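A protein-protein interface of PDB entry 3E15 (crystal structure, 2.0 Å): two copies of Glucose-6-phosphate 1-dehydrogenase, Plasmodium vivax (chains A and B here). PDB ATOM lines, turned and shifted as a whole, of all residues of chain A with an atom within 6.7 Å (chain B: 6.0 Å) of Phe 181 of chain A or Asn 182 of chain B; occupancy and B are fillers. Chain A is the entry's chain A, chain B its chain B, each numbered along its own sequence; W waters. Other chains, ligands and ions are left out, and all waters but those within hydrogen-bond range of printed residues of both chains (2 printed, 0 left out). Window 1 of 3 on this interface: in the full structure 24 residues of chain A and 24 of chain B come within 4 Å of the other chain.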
ATOM      1  N   PHE A 176      15.795   9.868  25.803  1.00  0.00           N
ATOM      2  CA  PHE A 176      15.324   8.562  25.340  1.00  0.00           C
ATOM      3  C   PHE A 176      13.931   8.708  24.744  1.00  0.00           C
ATOM      4  O   PHE A 176      13.043   9.225  25.395  1.00  0.00           O
ATOM      5  CB  PHE A 176      15.267   7.562  26.521  1.00  0.00           C
ATOM      6  CG  PHE A 176      16.618   7.085  26.940  1.00  0.00           C
ATOM      7  CD1 PHE A 176      17.236   6.061  26.254  1.00  0.00           C
ATOM      8  CD2 PHE A 176      17.295   7.691  27.991  1.00  0.00           C
ATOM      9  CE1 PHE A 176      18.491   5.638  26.603  1.00  0.00           C
ATOM     10  CE2 PHE A 176      18.563   7.262  28.344  1.00  0.00           C
ATOM     11  CZ  PHE A 176      19.158   6.246  27.643  1.00  0.00           C
ATOM     12  N   PRO A 177      13.739   8.232  23.502  1.00  0.00           N
ATOM     13  CA  PRO A 177      12.383   8.155  22.938  1.00  0.00           C
ATOM     14  C   PRO A 177      11.467   7.363  23.859  1.00  0.00           C
ATOM     15  O   PRO A 177      11.926   6.396  24.480  1.00  0.00           O
ATOM     16  CB  PRO A 177      12.612   7.409  21.611  1.00  0.00           C
ATOM     17  CG  PRO A 177      13.974   7.795  21.218  1.00  0.00           C
ATOM     18  CD  PRO A 177      14.752   7.786  22.517  1.00  0.00           C
ATOM     19  N   ASN A 178      10.201   7.763  24.004  1.00  0.00           N
ATOM     20  CA  ASN A 178       9.634   9.018  23.494  1.00  0.00           C
ATOM     21  C   ASN A 178       9.975  10.117  24.486  1.00  0.00           C
ATOM     22  O   ASN A 178       9.598  10.046  25.646  1.00  0.00           O
ATOM     23  CB  ASN A 178       8.100   8.867  23.392  1.00  0.00           C
ATOM     24  CG  ASN A 178       7.379  10.143  22.920  1.00  0.00           C
ATOM     25  OD1 ASN A 178       7.565  11.236  23.457  1.00  0.00           O
ATOM     26  ND2 ASN A 178       6.523   9.982  21.922  1.00  0.00           N
ATOM     27  N   ILE A 179      10.681  11.136  24.021  1.00  0.00           N
ATOM     28  CA  ILE A 179      11.302  12.114  24.907  1.00  0.00           C
ATOM     29  C   ILE A 179      10.243  12.873  25.674  1.00  0.00           C
ATOM     30  O   ILE A 179      10.410  13.164  26.859  1.00  0.00           O
ATOM     31  CB  ILE A 179      12.215  13.066  24.121  1.00  0.00           C
ATOM     32  CG1 ILE A 179      13.417  12.293  23.604  1.00  0.00           C
ATOM     33  CG2 ILE A 179      12.641  14.293  24.973  1.00  0.00           C
ATOM     34  CD1 ILE A 179      14.175  13.027  22.479  1.00  0.00           C
ATOM     35  N   PHE A 180       9.137  13.184  25.014  1.00  0.00           N
ATOM     36  CA  PHE A 180       8.031  13.862  25.704  1.00  0.00           C
ATOM     37  C   PHE A 180       7.378  12.984  26.789  1.00  0.00           C
ATOM     38  O   PHE A 180       7.150  13.435  27.906  1.00  0.00           O
ATOM     39  CB  PHE A 180       6.980  14.383  24.720  1.00  0.00           C
ATOM     40  CG  PHE A 180       5.801  14.999  25.406  1.00  0.00           C
ATOM     41  CD1 PHE A 180       5.955  16.141  26.173  1.00  0.00           C
ATOM     42  CD2 PHE A 180       4.552  14.434  25.310  1.00  0.00           C
ATOM     43  CE1 PHE A 180       4.869  16.705  26.829  1.00  0.00           C
ATOM     44  CE2 PHE A 180       3.467  15.006  25.965  1.00  0.00           C
ATOM     45  CZ  PHE A 180       3.640  16.133  26.722  1.00  0.00           C
ATOM     46  N   PHE A 181       7.083  11.723  26.477  1.00  0.00           N
ATOM     47  CA  PHE A 181       6.450  10.872  27.463  1.00  0.00           C
ATOM     48  C   PHE A 181       7.399  10.640  28.653  1.00  0.00           C
ATOM     49  O   PHE A 181       6.978  10.682  29.810  1.00  0.00           O
ATOM     50  CB  PHE A 181       6.087   9.510  26.885  1.00  0.00           C
ATOM     51  CG  PHE A 181       5.076   9.534  25.771  1.00  0.00           C
ATOM     52  CD1 PHE A 181       4.270  10.634  25.522  1.00  0.00           C
ATOM     53  CD2 PHE A 181       4.900   8.391  24.998  1.00  0.00           C
ATOM     54  CE1 PHE A 181       3.343  10.603  24.503  1.00  0.00           C
ATOM     55  CE2 PHE A 181       3.981   8.362  23.975  1.00  0.00           C
ATOM     56  CZ  PHE A 181       3.197   9.457  23.733  1.00  0.00           C
ATOM     57  N   ASN A 182       8.664  10.391  28.338  1.00  0.00           N
ATOM     58  CA  ASN A 182       9.672  10.033  29.314  1.00  0.00           C
ATOM     59  C   ASN A 182       9.942  11.233  30.237  1.00  0.00           C
ATOM     60  O   ASN A 182       9.891  11.101  31.451  1.00  0.00           O
ATOM     61  CB  ASN A 182      10.948   9.524  28.586  1.00  0.00           C
ATOM     62  CG  ASN A 182      11.983   8.880  29.541  1.00  0.00           C
ATOM     63  OD1 ASN A 182      12.410   9.493  30.519  1.00  0.00           O
ATOM     64  ND2 ASN A 182      12.363   7.654  29.253  1.00  0.00           N
ATOM     65  N   ILE A 183      10.164  12.413  29.664  1.00  0.00           N
ATOM     66  CA  ILE A 183      10.285  13.610  30.470  1.00  0.00           C
ATOM     67  C   ILE A 183       9.032  13.928  31.256  1.00  0.00           C
ATOM     68  O   ILE A 183       9.116  14.222  32.431  1.00  0.00           O
ATOM     69  CB  ILE A 183      10.743  14.816  29.660  1.00  0.00           C
ATOM     70  CG1 ILE A 183      12.199  14.584  29.207  1.00  0.00           C
ATOM     71  CG2 ILE A 183      10.619  16.115  30.500  1.00  0.00           C
ATOM     72  CD1 ILE A 183      12.786  15.671  28.282  1.00  0.00           C
ATOM     73  N   TYR A 184       7.860  13.885  30.624  1.00  0.00           N
ATOM     74  CA  TYR A 184       6.665  14.248  31.348  1.00  0.00           C
ATOM     75  C   TYR A 184       6.423  13.328  32.558  1.00  0.00           C
ATOM     76  O   TYR A 184       6.188  13.785  33.665  1.00  0.00           O
ATOM     77  CB  TYR A 184       5.433  14.267  30.439  1.00  0.00           C
ATOM     78  CG  TYR A 184       4.295  15.006  31.067  1.00  0.00           C
ATOM     79  CD1 TYR A 184       4.050  16.317  30.760  1.00  0.00           C
ATOM     80  CD2 TYR A 184       3.492  14.395  32.012  1.00  0.00           C
ATOM     81  CE1 TYR A 184       3.027  16.998  31.356  1.00  0.00           C
ATOM     82  CE2 TYR A 184       2.473  15.069  32.620  1.00  0.00           C
ATOM     83  CZ  TYR A 184       2.244  16.361  32.288  1.00  0.00           C
ATOM     84  OH  TYR A 184       1.225  17.041  32.888  1.00  0.00           O
ATOM     85  N   MET A 185       6.462  12.027  32.322  1.00  0.00           N
ATOM     86  CA  MET A 185       6.158  11.079  33.345  1.00  0.00           C
ATOM     87  C   MET A 185       7.193  11.131  34.469  1.00  0.00           C
ATOM     88  O   MET A 185       6.848  10.927  35.623  1.00  0.00           O
ATOM     89  CB  MET A 185       6.053   9.674  32.736  1.00  0.00           C
ATOM     90  CG  MET A 185       4.922   9.522  31.739  1.00  0.00           C
ATOM     91  SD  MET A 185       3.139   9.721  32.608  1.00  0.00           S
ATOM     92  CE  MET A 185       3.133   8.118  33.695  1.00  0.00           C
ATOM     93  N   ASN A 186       8.457  11.400  34.147  1.00  0.00           N
ATOM     94  CA  ASN A 186       9.495  11.403  35.183  1.00  0.00           C
ATOM     95  C   ASN A 186       9.632  12.749  35.964  1.00  0.00           C
ATOM     96  O   ASN A 186      10.185  12.766  37.049  1.00  0.00           O
ATOM     97  CB  ASN A 186      10.855  11.001  34.600  1.00  0.00           C
ATOM     98  CG  ASN A 186      10.995   9.522  34.412  1.00  0.00           C
ATOM     99  OD1 ASN A 186      10.719   8.739  35.318  1.00  0.00           O
ATOM    100  ND2 ASN A 186      11.454   9.115  33.219  1.00  0.00           N
ATOM    101  N   ASP A 209       3.428  15.437  19.120  1.00  0.00           N
ATOM    102  CA  ASP A 209       4.445  15.295  20.149  1.00  0.00           C
ATOM    103  C   ASP A 209       5.421  16.472  20.036  1.00  0.00           C
ATOM    104  O   ASP A 209       5.868  16.987  21.028  1.00  0.00           O
ATOM    105  CB  ASP A 209       5.217  13.987  20.012  1.00  0.00           C
ATOM    106  CG  ASP A 209       4.385  12.734  20.355  1.00  0.00           C
ATOM    107  OD1 ASP A 209       3.243  12.829  20.881  1.00  0.00           O
ATOM    108  OD2 ASP A 209       4.907  11.636  20.087  1.00  0.00           O
ATOM    109  N   ASN A 212       3.976  19.405  21.764  1.00  0.00           N
ATOM    110  CA  ASN A 212       4.002  19.113  23.198  1.00  0.00           C
ATOM    111  C   ASN A 212       5.442  19.242  23.817  1.00  0.00           C
ATOM    112  O   ASN A 212       5.626  19.799  24.892  1.00  0.00           O
ATOM    113  CB  ASN A 212       3.401  17.730  23.473  1.00  0.00           C
ATOM    114  CG  ASN A 212       1.887  17.768  23.662  1.00  0.00           C
ATOM    115  OD1 ASN A 212       1.332  18.764  24.114  1.00  0.00           O
ATOM    116  ND2 ASN A 212       1.223  16.662  23.345  1.00  0.00           N
ATOM    117  N   CYS A 274      10.603  13.720  19.153  1.00  0.00           N
ATOM    118  CA  CYS A 274      10.592  12.938  20.387  1.00  0.00           C
ATOM    119  C   CYS A 274      11.096  11.503  20.156  1.00  0.00           C
ATOM    120  O   CYS A 274      11.423  10.793  21.117  1.00  0.00           O
ATOM    121  CB  CYS A 274       9.204  12.881  20.958  1.00  0.00           C
ATOM    122  SG  CYS A 274       8.578  14.447  21.498  1.00  0.00           S
ATOM    123  N   SER B 174       1.815  -4.088  19.616  1.00  0.00           N
ATOM    124  CA  SER B 174       2.199  -2.660  19.567  1.00  0.00           C
ATOM    125  C   SER B 174       2.407  -2.098  20.977  1.00  0.00           C
ATOM    126  O   SER B 174       2.001  -0.982  21.306  1.00  0.00           O
ATOM    127  CB  SER B 174       1.173  -1.809  18.790  1.00  0.00           C
ATOM    128  OG  SER B 174       1.278  -2.052  17.376  1.00  0.00           O
ATOM    129  N   PHE B 176       4.952  -0.631  22.894  1.00  0.00           N
ATOM    130  CA  PHE B 176       6.229   0.070  22.680  1.00  0.00           C
ATOM    131  C   PHE B 176       6.789   0.568  24.003  1.00  0.00           C
ATOM    132  O   PHE B 176       6.097   1.283  24.756  1.00  0.00           O
ATOM    133  CB  PHE B 176       6.054   1.251  21.719  1.00  0.00           C
ATOM    134  CG  PHE B 176       5.803   0.839  20.310  1.00  0.00           C
ATOM    135  CD1 PHE B 176       6.874   0.532  19.463  1.00  0.00           C
ATOM    136  CD2 PHE B 176       4.515   0.740  19.826  1.00  0.00           C
ATOM    137  CE1 PHE B 176       6.655   0.133  18.171  1.00  0.00           C
ATOM    138  CE2 PHE B 176       4.271   0.341  18.531  1.00  0.00           C
ATOM    139  CZ  PHE B 176       5.335   0.029  17.694  1.00  0.00           C
ATOM    140  N   PRO B 177       8.027   0.176  24.313  1.00  0.00           N
ATOM    141  CA  PRO B 177       8.749   0.787  25.448  1.00  0.00           C
ATOM    142  C   PRO B 177       8.795   2.305  25.353  1.00  0.00           C
ATOM    143  O   PRO B 177       8.956   2.857  24.232  1.00  0.00           O
ATOM    144  CB  PRO B 177      10.163   0.198  25.314  1.00  0.00           C
ATOM    145  CG  PRO B 177       9.923  -1.168  24.687  1.00  0.00           C
ATOM    146  CD  PRO B 177       8.803  -0.917  23.689  1.00  0.00           C
ATOM    147  N   ASN B 178       8.642   3.016  26.469  1.00  0.00           N
ATOM    148  CA  ASN B 178       8.268   2.485  27.777  1.00  0.00           C
ATOM    149  C   ASN B 178       6.772   2.289  27.796  1.00  0.00           C
ATOM    150  O   ASN B 178       6.005   3.251  27.570  1.00  0.00           O
ATOM    151  CB  ASN B 178       8.725   3.485  28.862  1.00  0.00           C
ATOM    152  CG  ASN B 178       8.258   3.110  30.278  1.00  0.00           C
ATOM    153  OD1 ASN B 178       7.085   2.878  30.517  1.00  0.00           O
ATOM    154  ND2 ASN B 178       9.198   3.104  31.224  1.00  0.00           N
ATOM    155  N   ILE B 179       6.344   1.048  28.032  1.00  0.00           N
ATOM    156  CA  ILE B 179       4.949   0.684  27.829  1.00  0.00           C
ATOM    157  C   ILE B 179       4.019   1.449  28.776  1.00  0.00           C
ATOM    158  O   ILE B 179       2.961   1.911  28.373  1.00  0.00           O
ATOM    159  CB  ILE B 179       4.737  -0.845  27.964  1.00  0.00           C
ATOM    160  CG1 ILE B 179       5.343  -1.569  26.761  1.00  0.00           C
ATOM    161  CG2 ILE B 179       3.254  -1.193  28.086  1.00  0.00           C
ATOM    162  CD1 ILE B 179       5.607  -3.098  27.022  1.00  0.00           C
ATOM    163  N   PHE B 180       4.412   1.577  30.038  1.00  0.00           N
ATOM    164  CA  PHE B 180       3.625   2.369  30.959  1.00  0.00           C
ATOM    165  C   PHE B 180       3.508   3.865  30.566  1.00  0.00           C
ATOM    166  O   PHE B 180       2.398   4.415  30.562  1.00  0.00           O
ATOM    167  CB  PHE B 180       4.104   2.217  32.411  1.00  0.00           C
ATOM    168  CG  PHE B 180       3.263   2.986  33.362  1.00  0.00           C
ATOM    169  CD1 PHE B 180       1.966   2.594  33.598  1.00  0.00           C
ATOM    170  CD2 PHE B 180       3.728   4.130  33.957  1.00  0.00           C
ATOM    171  CE1 PHE B 180       1.148   3.322  34.471  1.00  0.00           C
ATOM    172  CE2 PHE B 180       2.906   4.860  34.816  1.00  0.00           C
ATOM    173  CZ  PHE B 180       1.627   4.446  35.051  1.00  0.00           C
ATOM    174  N   PHE B 181       4.633   4.513  30.236  1.00  0.00           N
ATOM    175  CA  PHE B 181       4.623   5.924  29.826  1.00  0.00           C
ATOM    176  C   PHE B 181       3.761   6.126  28.565  1.00  0.00           C
ATOM    177  O   PHE B 181       2.954   7.044  28.502  1.00  0.00           O
ATOM    178  CB  PHE B 181       6.043   6.450  29.502  1.00  0.00           C
ATOM    179  CG  PHE B 181       7.013   6.443  30.655  1.00  0.00           C
ATOM    180  CD1 PHE B 181       6.610   6.206  31.964  1.00  0.00           C
ATOM    181  CD2 PHE B 181       8.358   6.715  30.420  1.00  0.00           C
ATOM    182  CE1 PHE B 181       7.516   6.236  32.997  1.00  0.00           C
ATOM    183  CE2 PHE B 181       9.274   6.738  31.471  1.00  0.00           C
ATOM    184  CZ  PHE B 181       8.848   6.501  32.751  1.00  0.00           C
ATOM    185  N   ASN B 182       3.952   5.260  27.580  1.00  0.00           N
ATOM    186  CA  ASN B 182       3.253   5.357  26.293  1.00  0.00           C
ATOM    187  C   ASN B 182       1.753   5.145  26.458  1.00  0.00           C
ATOM    188  O   ASN B 182       0.970   5.918  25.973  1.00  0.00           O
ATOM    189  CB  ASN B 182       3.859   4.308  25.313  1.00  0.00           C
ATOM    190  CG  ASN B 182       3.450   4.516  23.881  1.00  0.00           C
ATOM    191  OD1 ASN B 182       2.271   4.537  23.575  1.00  0.00           O
ATOM    192  ND2 ASN B 182       4.438   4.628  22.970  1.00  0.00           N
ATOM    193  N   ILE B 183       1.363   4.092  27.165  1.00  0.00           N
ATOM    194  CA  ILE B 183      -0.034   3.853  27.448  1.00  0.00           C
ATOM    195  C   ILE B 183      -0.630   4.958  28.324  1.00  0.00           C
ATOM    196  O   ILE B 183      -1.715   5.460  28.021  1.00  0.00           O
ATOM    197  CB  ILE B 183      -0.281   2.445  28.054  1.00  0.00           C
ATOM    198  CG1 ILE B 183      -0.040   1.362  27.002  1.00  0.00           C
ATOM    199  CG2 ILE B 183      -1.721   2.315  28.642  1.00  0.00           C
ATOM    200  CD1 ILE B 183      -0.142  -0.078  27.543  1.00  0.00           C
ATOM    201  N   TYR B 184       0.064   5.371  29.397  1.00  0.00           N
ATOM    202  CA  TYR B 184      -0.492   6.426  30.250  1.00  0.00           C
ATOM    203  C   TYR B 184      -0.751   7.702  29.448  1.00  0.00           C
ATOM    204  O   TYR B 184      -1.847   8.289  29.490  1.00  0.00           O
ATOM    205  CB  TYR B 184       0.412   6.739  31.473  1.00  0.00           C
ATOM    206  CG  TYR B 184      -0.355   7.553  32.484  1.00  0.00           C
ATOM    207  CD1 TYR B 184      -1.058   6.933  33.490  1.00  0.00           C
ATOM    208  CD2 TYR B 184      -0.422   8.941  32.396  1.00  0.00           C
ATOM    209  CE1 TYR B 184      -1.779   7.647  34.397  1.00  0.00           C
ATOM    210  CE2 TYR B 184      -1.162   9.668  33.310  1.00  0.00           C
ATOM    211  CZ  TYR B 184      -1.832   9.012  34.306  1.00  0.00           C
ATOM    212  OH  TYR B 184      -2.576   9.708  35.233  1.00  0.00           O
ATOM    213  N   MET B 185       0.269   8.160  28.744  1.00  0.00           N
ATOM    214  CA  MET B 185       0.203   9.453  28.088  1.00  0.00           C
ATOM    215  C   MET B 185      -0.839   9.423  26.956  1.00  0.00           C
ATOM    216  O   MET B 185      -1.534  10.432  26.707  1.00  0.00           O
ATOM    217  CB  MET B 185       1.575   9.853  27.547  1.00  0.00           C
ATOM    218  CG  MET B 185       2.610  10.199  28.639  1.00  0.00           C
ATOM    219  SD  MET B 185       2.059  11.639  29.855  1.00  0.00           S
ATOM    220  CE  MET B 185       2.465  13.135  28.725  1.00  0.00           C
ATOM    221  N   ASN B 186      -0.966   8.282  26.280  1.00  0.00           N
ATOM    222  CA  ASN B 186      -1.927   8.180  25.157  1.00  0.00           C
ATOM    223  C   ASN B 186      -3.375   7.896  25.550  1.00  0.00           C
ATOM    224  O   ASN B 186      -4.286   8.168  24.763  1.00  0.00           O
ATOM    225  CB  ASN B 186      -1.471   7.142  24.131  1.00  0.00           C
ATOM    226  CG  ASN B 186      -0.367   7.650  23.244  1.00  0.00           C
ATOM    227  OD1 ASN B 186      -0.429   8.772  22.750  1.00  0.00           O
ATOM    228  ND2 ASN B 186       0.654   6.820  23.018  1.00  0.00           N
ATOM    229  N   ASN B 187      -3.595   7.318  26.731  1.00  0.00           N
ATOM    230  CA  ASN B 187      -4.915   6.774  27.098  1.00  0.00           C
ATOM    231  C   ASN B 187      -5.514   7.408  28.356  1.00  0.00           C
ATOM    232  O   ASN B 187      -6.728   7.605  28.443  1.00  0.00           O
ATOM    233  CB  ASN B 187      -4.860   5.258  27.305  1.00  0.00           C
ATOM    234  CG  ASN B 187      -4.518   4.496  26.032  1.00  0.00           C
ATOM    235  OD1 ASN B 187      -5.400   4.037  25.307  1.00  0.00           O
ATOM    236  ND2 ASN B 187      -3.243   4.344  25.774  1.00  0.00           N
ATOM    237  N   PHE B 222      -4.515   2.455  23.037  1.00  0.00           N
ATOM    238  CA  PHE B 222      -3.887   3.276  21.993  1.00  0.00           C
ATOM    239  C   PHE B 222      -2.385   3.411  22.304  1.00  0.00           C
ATOM    240  O   PHE B 222      -2.012   3.782  23.407  1.00  0.00           O
ATOM    241  CB  PHE B 222      -4.590   4.665  22.015  1.00  0.00           C
ATOM    242  CG  PHE B 222      -4.009   5.702  21.106  1.00  0.00           C
ATOM    243  CD1 PHE B 222      -3.486   5.378  19.874  1.00  0.00           C
ATOM    244  CD2 PHE B 222      -4.034   7.051  21.488  1.00  0.00           C
ATOM    245  CE1 PHE B 222      -2.979   6.370  19.057  1.00  0.00           C
ATOM    246  CE2 PHE B 222      -3.547   8.024  20.688  1.00  0.00           C
ATOM    247  CZ  PHE B 222      -3.001   7.703  19.478  1.00  0.00           C
ATOM    248  N   THR B 223      -1.532   3.093  21.343  1.00  0.00           N
ATOM    249  CA  THR B 223      -0.121   3.376  21.491  1.00  0.00           C
ATOM    250  C   THR B 223       0.397   4.113  20.272  1.00  0.00           C
ATOM    251  O   THR B 223      -0.252   4.131  19.231  1.00  0.00           O
ATOM    252  CB  THR B 223       0.723   2.071  21.763  1.00  0.00           C
ATOM    253  OG1 THR B 223       0.558   1.153  20.686  1.00  0.00           O
ATOM    254  CG2 THR B 223       0.311   1.384  23.115  1.00  0.00           C
ATOM    255  N   THR B 224       1.559   4.739  20.414  1.00  0.00           N
ATOM    256  CA  THR B 224       2.177   5.440  19.330  1.00  0.00           C
ATOM    257  C   THR B 224       3.632   5.058  19.105  1.00  0.00           C
ATOM    258  O   THR B 224       4.371   4.699  20.032  1.00  0.00           O
ATOM    259  CB  THR B 224       2.108   6.975  19.501  1.00  0.00           C
ATOM    260  OG1 THR B 224       2.703   7.358  20.743  1.00  0.00           O
ATOM    261  CG2 THR B 224       0.657   7.459  19.413  1.00  0.00           C
ATOM    262  N   THR B 225       4.032   5.178  17.848  1.00  0.00           N
ATOM    263  CA  THR B 225       5.408   5.013  17.427  1.00  0.00           C
ATOM    264  C   THR B 225       5.665   6.050  16.305  1.00  0.00           C
ATOM    265  O   THR B 225       4.921   7.033  16.182  1.00  0.00           O
ATOM    266  CB  THR B 225       5.660   3.552  16.958  1.00  0.00           C
ATOM    267  OG1 THR B 225       7.050   3.341  16.669  1.00  0.00           O
ATOM    268  CG2 THR B 225       4.804   3.198  15.736  1.00  0.00           C
HETATM  269  O   HOH W   1       5.630   7.537  20.524  1.00  0.00           O
HETATM  270  O   HOH W   2       2.701   9.997  20.580  1.00  0.00           O
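The side-chain sulfur (SD) of Met 185 of chain B lies close to the side-chain sulfur (SD) of Met 185 of chain A (3.5 Å).
N of Phe 180 of chain A lies within hydrogen-bond range of OD1 of Asn 178 of chain A (2.9 Å).
The side-chain amide oxygen of Asn 178 of chain A is in hydrogen-bond range of the backbone NH of Phe 181 of chain A, at 3.1 Å.
N of Phe 180 of chain A lies close to SG of Cys 274 of chain A (3.8 Å).
ND2 of Asn 186 of chain A lies within hydrogen-bond range of OD1 of Asn 182 of chain A (2.9 Å).
The backbone NH (N) of Phe 180 of chain B sits at hydrogen-bond distance from the side-chain amide oxygen (OD1) of Asn 178 of chain B (3.0 Å).
The side-chain amide nitrogen (ND2) of Asn 182 of chain B lies within hydrogen-bond range of the backbone carbonyl oxygen (O) of Thr 224 of chain B.
Among the printed residues, pairs that only touch across the chains: Met 185 of chain A with Phe 180 of chain B, Phe 181 of chain A with Met 185 of chain B, Phe 180 of chain A with Met 185 of chain B, Tyr 184 of chain A with Met 185 of chain B, Met 185 of chain A with Phe 181 of chain B, Phe 181 of chain A with Thr 224 of chain B, Met 185 of chain A with Tyr 184 of chain B, Asn 186 of chain A with Phe 181 of chain B, Phe 181 of chain A with Asn 182 of chain B, Phe 181 of chain A with Asn 186 of chain B and Asn 182 of chain A with Phe 181 of chain B.
Printed residues of chain B within 4 Å of Phe 181 of chain A: Asn 182 (3.7 Å), Met 185 (3.5 Å), Asn 186 (3.7 Å) and Thr 224 (3.6 Å).
Of the printed residues of chain B, Asn 182 of chain A touches Phe 181 (3.7 Å).
Of the printed residues of chain B, Met 185 of chain A touches Phe 180 (3.5 Å), Phe 181 (3.6 Å), Tyr 184 (3.7 Å) and Met 185 (3.5 Å).
Of the printed residues of chain B, Asn 186 of chain A touches Phe 181.
Asn 212 of chain A touches none of the printed residues of chain B.
Printed residues of chain A within 4 Å of Asn 182 of chain B: Phe 181.
Of the printed residues of chain A, Met 185 of chain B touches Phe 180, Phe 181, Tyr 184 and Met 185.
Thr 223 of chain B touches none of the printed residues of chain A.
Printed residues of chain A within 4 Å of Thr 224 of chain B: Phe 181 (3.6 Å).
The nearest residue of chain A that does not touch Asn 182 of chain B is Asn 178 of chain A (5.6 Å).
Of the 17 printed residues of chain B, 7 touch a printed residue of chain A.
Hydrophobic or aromatic side chains of chain A that line the printed part of chain B: Phe 180, Phe 181, Tyr 184 and Met 185.
Among the printed residues, no Asp or Glu carboxylate lies within 4 Å of a Lys or Arg side-chain nitrogen of the other chain.
Phe 180 of chain A touches Met 185 of chain B, and with the chains exchanged Met 185 of chain A touches Phe 180 of chain B.
Phe 181 of chain A touches Met 185 of chain B, and with the chains exchanged Met 185 of chain A touches Phe 181 of chain B.
Phe 181 of chain A touches Asn 186 of chain B, and with the chains exchanged Asn 186 of chain A touches Phe 181 of chain B.
Tyr 184 of chain A touches Met 185 of chain B, and with the chains exchanged Met 185 of chain A touches Tyr 184 of chain B.
Positions printed for both chains: 176, 177, 178, 179, 180, 181, 182, 183, 184, 185 and 186.
Of the 12 pairs that touch across the chains among the printed residues, 11 have their exchanged pair printed and touching as well.
Water W2 lies within hydrogen-bond range of the side-chain hydroxyl of Thr 224 of chain B (2.6 Å) and the side-chain carboxylate of Asp 209 of chain A (2.8 Å).
Water W1 lies within hydrogen-bond range of the side-chain hydroxyl of Thr 224 of chain B (2.9 Å) and the side-chain amide nitrogen of Asn 178 of chain A (3.0 Å).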
